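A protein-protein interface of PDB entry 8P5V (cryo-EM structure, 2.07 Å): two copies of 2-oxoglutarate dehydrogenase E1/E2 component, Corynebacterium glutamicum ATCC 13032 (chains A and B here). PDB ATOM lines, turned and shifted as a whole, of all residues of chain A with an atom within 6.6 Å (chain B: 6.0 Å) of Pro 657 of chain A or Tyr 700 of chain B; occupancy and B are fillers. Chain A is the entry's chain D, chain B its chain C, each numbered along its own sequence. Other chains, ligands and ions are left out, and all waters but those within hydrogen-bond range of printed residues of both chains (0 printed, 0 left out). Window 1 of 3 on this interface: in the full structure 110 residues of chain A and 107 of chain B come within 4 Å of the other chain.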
ATOM      1  N   ASN A 616       7.320  -9.825  -4.362  1.00  0.00           N
ATOM      2  CA  ASN A 616       6.026 -10.472  -4.232  1.00  0.00           C
ATOM      3  C   ASN A 616       5.731 -11.333  -5.458  1.00  0.00           C
ATOM      4  O   ASN A 616       5.493 -12.530  -5.312  1.00  0.00           O
ATOM      5  CB  ASN A 616       4.905  -9.468  -3.955  1.00  0.00           C
ATOM      6  CG  ASN A 616       5.047  -8.777  -2.617  1.00  0.00           C
ATOM      7  OD1 ASN A 616       6.083  -8.876  -1.967  1.00  0.00           O
ATOM      8  ND2 ASN A 616       4.018  -8.059  -2.204  1.00  0.00           N
ATOM      9  N   PHE A 650       2.853  -2.263   2.552  1.00  0.00           N
ATOM     10  CA  PHE A 650       1.706  -3.083   2.199  1.00  0.00           C
ATOM     11  C   PHE A 650       0.546  -2.190   1.761  1.00  0.00           C
ATOM     12  O   PHE A 650      -0.138  -2.510   0.795  1.00  0.00           O
ATOM     13  CB  PHE A 650       1.317  -4.005   3.359  1.00  0.00           C
ATOM     14  CG  PHE A 650       0.252  -5.017   3.025  1.00  0.00           C
ATOM     15  CD1 PHE A 650      -1.091  -4.702   3.133  1.00  0.00           C
ATOM     16  CD2 PHE A 650       0.595  -6.276   2.559  1.00  0.00           C
ATOM     17  CE1 PHE A 650      -2.066  -5.635   2.809  1.00  0.00           C
ATOM     18  CE2 PHE A 650      -0.378  -7.206   2.226  1.00  0.00           C
ATOM     19  CZ  PHE A 650      -1.708  -6.886   2.356  1.00  0.00           C
ATOM     20  N   ALA A 651       0.340  -1.078   2.475  1.00  0.00           N
ATOM     21  CA  ALA A 651      -0.720  -0.130   2.163  1.00  0.00           C
ATOM     22  C   ALA A 651      -0.316   0.753   0.979  1.00  0.00           C
ATOM     23  O   ALA A 651      -1.104   0.952   0.058  1.00  0.00           O
ATOM     24  CB  ALA A 651      -1.036   0.706   3.382  1.00  0.00           C
ATOM     25  N   LEU A 653       2.422   0.692  -1.535  1.00  0.00           N
ATOM     26  CA  LEU A 653       2.777   0.212  -2.861  1.00  0.00           C
ATOM     27  C   LEU A 653       1.607  -0.551  -3.473  1.00  0.00           C
ATOM     28  O   LEU A 653       0.847  -1.206  -2.763  1.00  0.00           O
ATOM     29  CB  LEU A 653       4.011  -0.695  -2.791  1.00  0.00           C
ATOM     30  CG  LEU A 653       5.353  -0.002  -2.593  1.00  0.00           C
ATOM     31  CD1 LEU A 653       5.524   1.168  -3.550  1.00  0.00           C
ATOM     32  CD2 LEU A 653       5.520   0.447  -1.162  1.00  0.00           C
ATOM     33  N   GLY A 654       1.512  -0.485  -4.807  1.00  0.00           N
ATOM     34  CA  GLY A 654       0.408  -1.063  -5.548  1.00  0.00           C
ATOM     35  C   GLY A 654       0.700  -2.466  -6.075  1.00  0.00           C
ATOM     36  O   GLY A 654      -0.220  -3.188  -6.456  1.00  0.00           O
ATOM     37  N   ILE A 655       1.980  -2.854  -6.090  1.00  0.00           N
ATOM     38  CA  ILE A 655       2.368  -4.189  -6.527  1.00  0.00           C
ATOM     39  C   ILE A 655       1.772  -5.238  -5.584  1.00  0.00           C
ATOM     40  O   ILE A 655       1.559  -6.379  -5.985  1.00  0.00           O
ATOM     41  CB  ILE A 655       3.904  -4.310  -6.648  1.00  0.00           C
ATOM     42  CG1 ILE A 655       4.337  -5.659  -7.230  1.00  0.00           C
ATOM     43  CG2 ILE A 655       4.597  -4.039  -5.321  1.00  0.00           C
ATOM     44  CD1 ILE A 655       3.685  -6.015  -8.542  1.00  0.00           C
ATOM     45  N   VAL A 656       1.490  -4.843  -4.338  1.00  0.00           N
ATOM     46  CA  VAL A 656       0.970  -5.761  -3.339  1.00  0.00           C
ATOM     47  C   VAL A 656      -0.383  -6.312  -3.784  1.00  0.00           C
ATOM     48  O   VAL A 656      -0.504  -7.513  -4.021  1.00  0.00           O
ATOM     49  CB  VAL A 656       0.910  -5.103  -1.951  1.00  0.00           C
ATOM     50  CG1 VAL A 656       0.158  -5.966  -0.953  1.00  0.00           C
ATOM     51  CG2 VAL A 656       2.302  -4.778  -1.445  1.00  0.00           C
ATOM     52  N   PRO A 657      -1.449  -5.486  -3.917  1.00  0.00           N
ATOM     53  CA  PRO A 657      -2.738  -5.997  -4.382  1.00  0.00           C
ATOM     54  C   PRO A 657      -2.675  -6.553  -5.801  1.00  0.00           C
ATOM     55  O   PRO A 657      -3.443  -7.444  -6.158  1.00  0.00           O
ATOM     56  CB  PRO A 657      -3.671  -4.780  -4.294  1.00  0.00           C
ATOM     57  CG  PRO A 657      -2.748  -3.585  -4.317  1.00  0.00           C
ATOM     58  CD  PRO A 657      -1.495  -4.048  -3.610  1.00  0.00           C
ATOM     59  N   GLU A 658      -1.735  -6.036  -6.597  1.00  0.00           N
ATOM     60  CA  GLU A 658      -1.548  -6.492  -7.962  1.00  0.00           C
ATOM     61  C   GLU A 658      -1.170  -7.973  -7.977  1.00  0.00           C
ATOM     62  O   GLU A 658      -1.650  -8.722  -8.822  1.00  0.00           O
ATOM     63  CB  GLU A 658      -0.493  -5.616  -8.641  1.00  0.00           C
ATOM     64  CG  GLU A 658      -0.301  -5.906 -10.115  1.00  0.00           C
ATOM     65  CD  GLU A 658       0.578  -4.897 -10.837  1.00  0.00           C
ATOM     66  OE1 GLU A 658       1.072  -3.956 -10.175  1.00  0.00           O
ATOM     67  OE2 GLU A 658       0.769  -5.054 -12.058  1.00  0.00           O
ATOM     68  N   THR A 659      -0.305  -8.394  -7.045  1.00  0.00           N
ATOM     69  CA  THR A 659       0.146  -9.777  -7.001  1.00  0.00           C
ATOM     70  C   THR A 659      -0.925 -10.665  -6.371  1.00  0.00           C
ATOM     71  O   THR A 659      -1.144 -11.782  -6.829  1.00  0.00           O
ATOM     72  CB  THR A 659       1.481  -9.903  -6.261  1.00  0.00           C
ATOM     73  OG1 THR A 659       2.393  -8.997  -6.884  1.00  0.00           O
ATOM     74  CG2 THR A 659       2.040 -11.309  -6.292  1.00  0.00           C
ATOM     75  N   ILE A 660      -1.591 -10.168  -5.323  1.00  0.00           N
ATOM     76  CA  ILE A 660      -2.640 -10.930  -4.663  1.00  0.00           C
ATOM     77  C   ILE A 660      -3.731 -11.263  -5.675  1.00  0.00           C
ATOM     78  O   ILE A 660      -4.386 -12.296  -5.574  1.00  0.00           O
ATOM     79  CB  ILE A 660      -3.213 -10.172  -3.454  1.00  0.00           C
ATOM     80  CG1 ILE A 660      -2.151  -9.919  -2.384  1.00  0.00           C
ATOM     81  CG2 ILE A 660      -4.416 -10.914  -2.891  1.00  0.00           C
ATOM     82  CD1 ILE A 660      -2.538  -8.878  -1.372  1.00  0.00           C
ATOM     83  N   ASN A 661      -3.893 -10.381  -6.663  1.00  0.00           N
ATOM     84  CA  ASN A 661      -4.896 -10.529  -7.697  1.00  0.00           C
ATOM     85  C   ASN A 661      -4.653 -11.788  -8.529  1.00  0.00           C
ATOM     86  O   ASN A 661      -5.578 -12.280  -9.167  1.00  0.00           O
ATOM     87  CB  ASN A 661      -4.936  -9.267  -8.562  1.00  0.00           C
ATOM     88  CG  ASN A 661      -6.156  -9.205  -9.446  1.00  0.00           C
ATOM     89  OD1 ASN A 661      -7.274  -9.222  -8.944  1.00  0.00           O
ATOM     90  ND2 ASN A 661      -5.945  -9.155 -10.752  1.00  0.00           N
ATOM     91  N   LEU A 662      -3.423 -12.321  -8.522  1.00  0.00           N
ATOM     92  CA  LEU A 662      -3.094 -13.504  -9.309  1.00  0.00           C
ATOM     93  C   LEU A 662      -3.423 -14.801  -8.562  1.00  0.00           C
ATOM     94  O   LEU A 662      -3.274 -15.878  -9.131  1.00  0.00           O
ATOM     95  CB  LEU A 662      -1.603 -13.467  -9.665  1.00  0.00           C
ATOM     96  CG  LEU A 662      -1.125 -12.272 -10.490  1.00  0.00           C
ATOM     97  CD1 LEU A 662       0.349 -12.422 -10.825  1.00  0.00           C
ATOM     98  CD2 LEU A 662      -1.933 -12.116 -11.768  1.00  0.00           C
ATOM     99  N   MET A 694      -6.867   3.645   4.634  1.00  0.00           N
ATOM    100  CA  MET A 694      -7.567   2.491   5.173  1.00  0.00           C
ATOM    101  C   MET A 694      -7.438   2.503   6.691  1.00  0.00           C
ATOM    102  O   MET A 694      -6.495   3.085   7.221  1.00  0.00           O
ATOM    103  CB  MET A 694      -6.958   1.194   4.641  1.00  0.00           C
ATOM    104  CG  MET A 694      -7.044   1.061   3.146  1.00  0.00           C
ATOM    105  SD  MET A 694      -6.059  -0.326   2.520  1.00  0.00           S
ATOM    106  CE  MET A 694      -4.439   0.112   3.152  1.00  0.00           C
ATOM    107  N   ASP A 699      -6.297  -4.237   4.945  1.00  0.00           N
ATOM    108  CA  ASP A 699      -7.671  -4.096   4.485  1.00  0.00           C
ATOM    109  C   ASP A 699      -7.831  -4.560   3.038  1.00  0.00           C
ATOM    110  O   ASP A 699      -8.957  -4.771   2.595  1.00  0.00           O
ATOM    111  CB  ASP A 699      -8.177  -2.665   4.670  1.00  0.00           C
ATOM    112  CG  ASP A 699      -8.856  -2.420   6.011  1.00  0.00           C
ATOM    113  OD1 ASP A 699      -9.321  -3.404   6.629  1.00  0.00           O
ATOM    114  OD2 ASP A 699      -8.887  -1.247   6.441  1.00  0.00           O
ATOM    115  N   TYR A 700      -6.723  -4.762   2.313  1.00  0.00           N
ATOM    116  CA  TYR A 700      -6.793  -5.312   0.969  1.00  0.00           C
ATOM    117  C   TYR A 700      -7.410  -6.710   0.975  1.00  0.00           C
ATOM    118  O   TYR A 700      -7.962  -7.138  -0.033  1.00  0.00           O
ATOM    119  CB  TYR A 700      -5.415  -5.330   0.300  1.00  0.00           C
ATOM    120  CG  TYR A 700      -4.907  -3.973  -0.111  1.00  0.00           C
ATOM    121  CD1 TYR A 700      -5.591  -3.209  -1.044  1.00  0.00           C
ATOM    122  CD2 TYR A 700      -3.754  -3.436   0.439  1.00  0.00           C
ATOM    123  CE1 TYR A 700      -5.141  -1.953  -1.422  1.00  0.00           C
ATOM    124  CE2 TYR A 700      -3.295  -2.179   0.078  1.00  0.00           C
ATOM    125  CZ  TYR A 700      -3.989  -1.433  -0.857  1.00  0.00           C
ATOM    126  OH  TYR A 700      -3.530  -0.186  -1.216  1.00  0.00           O
ATOM    127  N   ALA A 703     -10.967  -6.967  -0.053  1.00  0.00           N
ATOM    128  CA  ALA A 703     -11.186  -6.941  -1.486  1.00  0.00           C
ATOM    129  C   ALA A 703     -11.217  -8.359  -2.047  1.00  0.00           C
ATOM    130  O   ALA A 703     -12.052  -8.672  -2.897  1.00  0.00           O
ATOM    131  CB  ALA A 703     -10.125  -6.100  -2.150  1.00  0.00           C
ATOM    132  N   PHE A 704     -10.327  -9.226  -1.550  1.00  0.00           N
ATOM    133  CA  PHE A 704     -10.140 -10.548  -2.130  1.00  0.00           C
ATOM    134  C   PHE A 704     -10.934 -11.610  -1.374  1.00  0.00           C
ATOM    135  O   PHE A 704     -10.914 -12.774  -1.757  1.00  0.00           O
ATOM    136  CB  PHE A 704      -8.650 -10.886  -2.168  1.00  0.00           C
ATOM    137  CG  PHE A 704      -7.843  -9.892  -2.961  1.00  0.00           C
ATOM    138  CD1 PHE A 704      -7.794  -9.958  -4.342  1.00  0.00           C
ATOM    139  CD2 PHE A 704      -7.187  -8.855  -2.326  1.00  0.00           C
ATOM    140  CE1 PHE A 704      -7.074  -9.024  -5.068  1.00  0.00           C
ATOM    141  CE2 PHE A 704      -6.468  -7.920  -3.055  1.00  0.00           C
ATOM    142  CZ  PHE A 704      -6.410  -8.008  -4.424  1.00  0.00           C
ATOM    143  N   PHE B 650      -8.616  -1.625 -13.423  1.00  0.00           N
ATOM    144  CA  PHE B 650      -8.913  -1.245 -12.052  1.00  0.00           C
ATOM    145  C   PHE B 650      -8.473  -2.354 -11.099  1.00  0.00           C
ATOM    146  O   PHE B 650      -7.912  -2.068 -10.044  1.00  0.00           O
ATOM    147  CB  PHE B 650     -10.396  -0.902 -11.889  1.00  0.00           C
ATOM    148  CG  PHE B 650     -10.759  -0.327 -10.543  1.00  0.00           C
ATOM    149  CD1 PHE B 650     -11.071  -1.150  -9.473  1.00  0.00           C
ATOM    150  CD2 PHE B 650     -10.751   1.041 -10.334  1.00  0.00           C
ATOM    151  CE1 PHE B 650     -11.391  -0.616  -8.234  1.00  0.00           C
ATOM    152  CE2 PHE B 650     -11.068   1.576  -9.096  1.00  0.00           C
ATOM    153  CZ  PHE B 650     -11.389   0.746  -8.049  1.00  0.00           C
ATOM    154  N   ALA B 651      -8.730  -3.610 -11.484  1.00  0.00           N
ATOM    155  CA  ALA B 651      -8.362  -4.762 -10.677  1.00  0.00           C
ATOM    156  C   ALA B 651      -6.873  -5.070 -10.828  1.00  0.00           C
ATOM    157  O   ALA B 651      -6.183  -5.296  -9.837  1.00  0.00           O
ATOM    158  CB  ALA B 651      -9.201  -5.946 -11.079  1.00  0.00           C
ATOM    159  N   GLY B 652      -6.393  -5.074 -12.079  1.00  0.00           N
ATOM    160  CA  GLY B 652      -5.034  -5.477 -12.402  1.00  0.00           C
ATOM    161  C   GLY B 652      -3.983  -4.539 -11.814  1.00  0.00           C
ATOM    162  O   GLY B 652      -3.212  -4.937 -10.948  1.00  0.00           O
ATOM    163  N   LEU B 653      -3.968  -3.289 -12.288  1.00  0.00           N
ATOM    164  CA  LEU B 653      -2.878  -2.372 -11.992  1.00  0.00           C
ATOM    165  C   LEU B 653      -2.932  -1.943 -10.534  1.00  0.00           C
ATOM    166  O   LEU B 653      -4.006  -1.854  -9.947  1.00  0.00           O
ATOM    167  CB  LEU B 653      -2.947  -1.161 -12.928  1.00  0.00           C
ATOM    168  CG  LEU B 653      -2.554  -1.429 -14.384  1.00  0.00           C
ATOM    169  CD1 LEU B 653      -2.948  -0.260 -15.270  1.00  0.00           C
ATOM    170  CD2 LEU B 653      -1.063  -1.717 -14.537  1.00  0.00           C
ATOM    171  N   GLY B 654      -1.751  -1.667  -9.974  1.00  0.00           N
ATOM    172  CA  GLY B 654      -1.591  -1.383  -8.559  1.00  0.00           C
ATOM    173  C   GLY B 654      -1.595   0.110  -8.237  1.00  0.00           C
ATOM    174  O   GLY B 654      -1.768   0.496  -7.082  1.00  0.00           O
ATOM    175  N   VAL B 656      -3.861   2.027  -8.930  1.00  0.00           N
ATOM    176  CA  VAL B 656      -5.233   2.360  -8.590  1.00  0.00           C
ATOM    177  C   VAL B 656      -5.392   2.443  -7.072  1.00  0.00           C
ATOM    178  O   VAL B 656      -5.680   3.517  -6.548  1.00  0.00           O
ATOM    179  CB  VAL B 656      -6.224   1.374  -9.234  1.00  0.00           C
ATOM    180  CG1 VAL B 656      -7.632   1.566  -8.701  1.00  0.00           C
ATOM    181  CG2 VAL B 656      -6.194   1.485 -10.750  1.00  0.00           C
ATOM    182  N   PRO B 657      -5.221   1.341  -6.303  1.00  0.00           N
ATOM    183  CA  PRO B 657      -5.328   1.420  -4.848  1.00  0.00           C
ATOM    184  C   PRO B 657      -4.271   2.327  -4.224  1.00  0.00           C
ATOM    185  O   PRO B 657      -4.492   2.910  -3.165  1.00  0.00           O
ATOM    186  CB  PRO B 657      -5.167  -0.035  -4.383  1.00  0.00           C
ATOM    187  CG  PRO B 657      -4.450  -0.721  -5.522  1.00  0.00           C
ATOM    188  CD  PRO B 657      -4.946  -0.027  -6.770  1.00  0.00           C
ATOM    189  N   ILE B 660      -5.830   5.792  -4.372  1.00  0.00           N
ATOM    190  CA  ILE B 660      -6.973   5.871  -3.476  1.00  0.00           C
ATOM    191  C   ILE B 660      -6.477   6.021  -2.042  1.00  0.00           C
ATOM    192  O   ILE B 660      -7.133   6.647  -1.215  1.00  0.00           O
ATOM    193  CB  ILE B 660      -7.894   4.646  -3.618  1.00  0.00           C
ATOM    194  CG1 ILE B 660      -8.480   4.545  -5.030  1.00  0.00           C
ATOM    195  CG2 ILE B 660      -8.987   4.689  -2.563  1.00  0.00           C
ATOM    196  CD1 ILE B 660      -9.068   3.198  -5.353  1.00  0.00           C
ATOM    197  N   MET B 694     -10.588 -11.133  -7.171  1.00  0.00           N
ATOM    198  CA  MET B 694     -11.695 -10.540  -6.440  1.00  0.00           C
ATOM    199  C   MET B 694     -12.998 -10.924  -7.129  1.00  0.00           C
ATOM    200  O   MET B 694     -13.001 -11.220  -8.321  1.00  0.00           O
ATOM    201  CB  MET B 694     -11.579  -9.016  -6.433  1.00  0.00           C
ATOM    202  CG  MET B 694     -10.329  -8.515  -5.764  1.00  0.00           C
ATOM    203  SD  MET B 694     -10.070  -6.740  -6.018  1.00  0.00           S
ATOM    204  CE  MET B 694     -10.060  -6.676  -7.808  1.00  0.00           C
ATOM    205  N   TYR B 696     -15.692  -8.805  -7.279  1.00  0.00           N
ATOM    206  CA  TYR B 696     -15.998  -7.584  -8.010  1.00  0.00           C
ATOM    207  C   TYR B 696     -14.715  -6.817  -8.306  1.00  0.00           C
ATOM    208  O   TYR B 696     -13.771  -6.856  -7.521  1.00  0.00           O
ATOM    209  CB  TYR B 696     -16.911  -6.664  -7.200  1.00  0.00           C
ATOM    210  CG  TYR B 696     -18.299  -7.185  -6.943  1.00  0.00           C
ATOM    211  CD1 TYR B 696     -19.122  -7.569  -7.986  1.00  0.00           C
ATOM    212  CD2 TYR B 696     -18.806  -7.260  -5.656  1.00  0.00           C
ATOM    213  CE1 TYR B 696     -20.408  -8.027  -7.760  1.00  0.00           C
ATOM    214  CE2 TYR B 696     -20.093  -7.714  -5.414  1.00  0.00           C
ATOM    215  CZ  TYR B 696     -20.899  -8.095  -6.469  1.00  0.00           C
ATOM    216  OH  TYR B 696     -22.166  -8.549  -6.199  1.00  0.00           O
ATOM    217  N   ALA B 697     -14.715  -6.088  -9.425  1.00  0.00           N
ATOM    218  CA  ALA B 697     -13.593  -5.244  -9.791  1.00  0.00           C
ATOM    219  C   ALA B 697     -13.431  -4.119  -8.769  1.00  0.00           C
ATOM    220  O   ALA B 697     -12.311  -3.751  -8.429  1.00  0.00           O
ATOM    221  CB  ALA B 697     -13.791  -4.705 -11.184  1.00  0.00           C
ATOM    222  N   THR B 698     -14.552  -3.616  -8.240  1.00  0.00           N
ATOM    223  CA  THR B 698     -14.545  -2.463  -7.355  1.00  0.00           C
ATOM    224  C   THR B 698     -14.309  -2.861  -5.898  1.00  0.00           C
ATOM    225  O   THR B 698     -14.552  -2.061  -4.996  1.00  0.00           O
ATOM    226  CB  THR B 698     -15.862  -1.686  -7.467  1.00  0.00           C
ATOM    227  OG1 THR B 698     -16.901  -2.629  -7.199  1.00  0.00           O
ATOM    228  CG2 THR B 698     -16.060  -1.037  -8.819  1.00  0.00           C
ATOM    229  N   ASP B 699     -13.798  -4.074  -5.659  1.00  0.00           N
ATOM    230  CA  ASP B 699     -13.692  -4.603  -4.307  1.00  0.00           C
ATOM    231  C   ASP B 699     -12.635  -3.859  -3.491  1.00  0.00           C
ATOM    232  O   ASP B 699     -12.618  -3.988  -2.269  1.00  0.00           O
ATOM    233  CB  ASP B 699     -13.423  -6.109  -4.316  1.00  0.00           C
ATOM    234  CG  ASP B 699     -14.681  -6.962  -4.289  1.00  0.00           C
ATOM    235  OD1 ASP B 699     -15.729  -6.455  -3.841  1.00  0.00           O
ATOM    236  OD2 ASP B 699     -14.615  -8.119  -4.736  1.00  0.00           O
ATOM    237  N   TYR B 700     -11.787  -3.056  -4.145  1.00  0.00           N
ATOM    238  CA  TYR B 700     -10.829  -2.226  -3.432  1.00  0.00           C
ATOM    239  C   TYR B 700     -11.536  -1.241  -2.503  1.00  0.00           C
ATOM    240  O   TYR B 700     -10.947  -0.803  -1.522  1.00  0.00           O
ATOM    241  CB  TYR B 700      -9.902  -1.485  -4.401  1.00  0.00           C
ATOM    242  CG  TYR B 700      -8.875  -2.364  -5.069  1.00  0.00           C
ATOM    243  CD1 TYR B 700      -7.927  -3.045  -4.321  1.00  0.00           C
ATOM    244  CD2 TYR B 700      -8.862  -2.537  -6.444  1.00  0.00           C
ATOM    245  CE1 TYR B 700      -6.991  -3.871  -4.921  1.00  0.00           C
ATOM    246  CE2 TYR B 700      -7.936  -3.364  -7.059  1.00  0.00           C
ATOM    247  CZ  TYR B 700      -6.991  -4.028  -6.297  1.00  0.00           C
ATOM    248  OH  TYR B 700      -6.068  -4.848  -6.908  1.00  0.00           O
ATOM    249  N   ALA B 701     -12.793  -0.893  -2.806  1.00  0.00           N
ATOM    250  CA  ALA B 701     -13.557   0.035  -1.988  1.00  0.00           C
ATOM    251  C   ALA B 701     -13.759  -0.504  -0.574  1.00  0.00           C
ATOM    252  O   ALA B 701     -13.831   0.273   0.376  1.00  0.00           O
ATOM    253  CB  ALA B 701     -14.883   0.305  -2.643  1.00  0.00           C
ATOM    254  N   LYS B 702     -13.875  -1.834  -0.441  1.00  0.00           N
ATOM    255  CA  LYS B 702     -14.024  -2.455   0.865  1.00  0.00           C
ATOM    256  C   LYS B 702     -12.804  -2.178   1.731  1.00  0.00           C
ATOM    257  O   LYS B 702     -12.939  -2.015   2.938  1.00  0.00           O
ATOM    258  CB  LYS B 702     -14.269  -3.949   0.709  1.00  0.00           C
ATOM    259  CG  LYS B 702     -15.697  -4.247   0.277  1.00  0.00           C
ATOM    260  CD  LYS B 702     -15.818  -5.345  -0.727  1.00  0.00           C
ATOM    261  CE  LYS B 702     -17.203  -5.954  -0.712  1.00  0.00           C
ATOM    262  NZ  LYS B 702     -17.438  -6.813  -1.896  1.00  0.00           N
ATOM    263  N   ALA B 703     -11.629  -2.118   1.102  1.00  0.00           N
ATOM    264  CA  ALA B 703     -10.402  -1.828   1.822  1.00  0.00           C
ATOM    265  C   ALA B 703     -10.458  -0.436   2.449  1.00  0.00           C
ATOM    266  O   ALA B 703     -10.039  -0.253   3.591  1.00  0.00           O
ATOM    267  CB  ALA B 703      -9.215  -1.975   0.901  1.00  0.00           C
ATOM    268  N   PHE B 704     -11.009   0.534   1.713  1.00  0.00           N
ATOM    269  CA  PHE B 704     -10.958   1.929   2.126  1.00  0.00           C
ATOM    270  C   PHE B 704     -12.243   2.352   2.833  1.00  0.00           C
ATOM    271  O   PHE B 704     -12.356   3.494   3.269  1.00  0.00           O
ATOM    272  CB  PHE B 704     -10.670   2.820   0.918  1.00  0.00           C
ATOM    273  CG  PHE B 704      -9.387   2.469   0.216  1.00  0.00           C
ATOM    274  CD1 PHE B 704      -9.340   1.423  -0.687  1.00  0.00           C
ATOM    275  CD2 PHE B 704      -8.214   3.143   0.503  1.00  0.00           C
ATOM    276  CE1 PHE B 704      -8.154   1.082  -1.319  1.00  0.00           C
ATOM    277  CE2 PHE B 704      -7.034   2.811  -0.141  1.00  0.00           C
ATOM    278  CZ  PHE B 704      -7.000   1.769  -1.033  1.00  0.00           C
ATOM    279  N   GLY B 705     -13.203   1.430   2.957  1.00  0.00           N
ATOM    280  CA  GLY B 705     -14.420   1.698   3.703  1.00  0.00           C
ATOM    281  C   GLY B 705     -15.325   2.687   2.975  1.00  0.00           C
ATOM    282  O   GLY B 705     -15.874   3.597   3.586  1.00  0.00           O
ATOM    283  N   PHE B 738     -17.659   4.649  -5.230  1.00  0.00           N
ATOM    284  CA  PHE B 738     -17.340   3.799  -6.365  1.00  0.00           C
ATOM    285  C   PHE B 738     -18.621   3.352  -7.052  1.00  0.00           C
ATOM    286  O   PHE B 738     -19.523   2.834  -6.403  1.00  0.00           O
ATOM    287  CB  PHE B 738     -16.515   2.591  -5.921  1.00  0.00           C
ATOM    288  CG  PHE B 738     -15.157   2.949  -5.381  1.00  0.00           C
ATOM    289  CD1 PHE B 738     -15.015   3.447  -4.098  1.00  0.00           C
ATOM    290  CD2 PHE B 738     -14.032   2.862  -6.185  1.00  0.00           C
ATOM    291  CE1 PHE B 738     -13.771   3.818  -3.616  1.00  0.00           C
ATOM    292  CE2 PHE B 738     -12.789   3.227  -5.698  1.00  0.00           C
ATOM    293  CZ  PHE B 738     -12.662   3.704  -4.416  1.00  0.00           C
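The side-chain carboxylate (OD2) of Asp 699 of chain B sits close to the backbone carbonyl oxygen (O) of Ala 703 of chain A.
The backbone carbonyl oxygen (O) of Ala 703 of chain B sits close to the side-chain carboxylate (OD2) of Asp 699 of chain A (3.2 Å).
Printed residues of chain A that touch a printed residue of chain B: Gly 654, Pro 657, Glu 658, Asn 661, Met 694, Asp 699, Tyr 700, Ala 703 and Phe 704.
Hydrophobic or aromatic side chains of chain A within 4 Å of the printed part of chain B: Pro 657, Met 694, Tyr 700, Ala 703 and Phe 704.
Among the printed residues, no Asp or Glu carboxylate lies within 4 Å of a Lys or Arg side-chain nitrogen of the other chain.
Of the printed residues of chain B, Pro 657 of chain A touches Pro 657 (3.5 Å) and Tyr 700 (3.5 Å).
Of the printed residues of chain B, Tyr 700 of chain A touches Pro 657 (3.5 Å), Ala 703 (3.996 Å) and Phe 704 (3.99 Å).
Of the printed residues of chain B, Ala 703 of chain A touches Met 694 and Asp 699.
Printed residues of chain A within 4 Å of Ala 651 of chain B: Asn 661.
Of the printed residues of chain A, Tyr 700 of chain B touches Pro 657 (3.5 Å).
Ala 701 of chain B touches none of the printed residues of chain A.
The nearest printed residue of chain A that does not touch Tyr 700 of chain B is Ala 703 of chain A (4.001 Å).
Gly 654 of chain A touches its own counterpart, Gly 654 of chain B.
Met 694 of chain A touches Phe 704 of chain B, and with the chains exchanged Phe 704 of chain A touches Met 694 of chain B.
Tyr 700 of chain A touches Ala 703 of chain B, but with the chains exchanged Ala 703 of chain A does not touch Tyr 700 of chain B (4.001 Å).
Tyr 700 of chain A touches Phe 704 of chain B, but with the chains exchanged Phe 704 of chain A does not touch Tyr 700 of chain B (4.03 Å).
12 positions are printed for both chains.
Of the 16 pairs that touch across the chains among the printed residues, 10 have their exchanged pair printed and touching as well.
Among the printed residues, pairs that only touch across the chains: Gly 654 of chain A with Gly 654 of chain B (3.1 Å), Pro 657 of chain A with Pro 657 of chain B (3.5 Å), Pro 657 of chain A with Tyr 700 of chain B (3.5 Å), Glu 658 of chain A with Gly 652 of chain B (3.2 Å), Glu 658 of chain A with Gly 654 of chain B (3.6 Å), Asn 661 of chain A with Ala 651 of chain B (3.9 Å), Asn 661 of chain A with Met 694 of chain B (3.9 Å), Met 694 of chain A with Ala 703 of chain B (3.3 Å), Met 694 of chain A with Phe 704 of chain B (3.6 Å), Tyr 700 of chain A with Pro 657 of chain B (3.5 Å), Tyr 700 of chain A with Ala 703 of chain B (3.996 Å), Tyr 700 of chain A with Phe 704 of chain B (3.99 Å), Ala 703 of chain A with Met 694 of chain B (3.3 Å) and Phe 704 of chain A with Met 694 of chain B (3.2 Å).
OD1 of Asp 699 of chain B is in salt-bridge range of NZ of Lys 702 of chain B, 2.6 Å away.
O of Ala 651 of chain A sits at hydrogen-bond distance from OH of Tyr 700 of chain A (3.0 Å).
The backbone carbonyl oxygen of Ala 651 of chain B is in hydrogen-bond range of the side-chain hydroxyl of Tyr 700 of chain B (3.0 Å).
N of Tyr 696 of chain B lies within hydrogen-bond range of OD2 of Asp 699 of chain B, at 2.8 Å.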
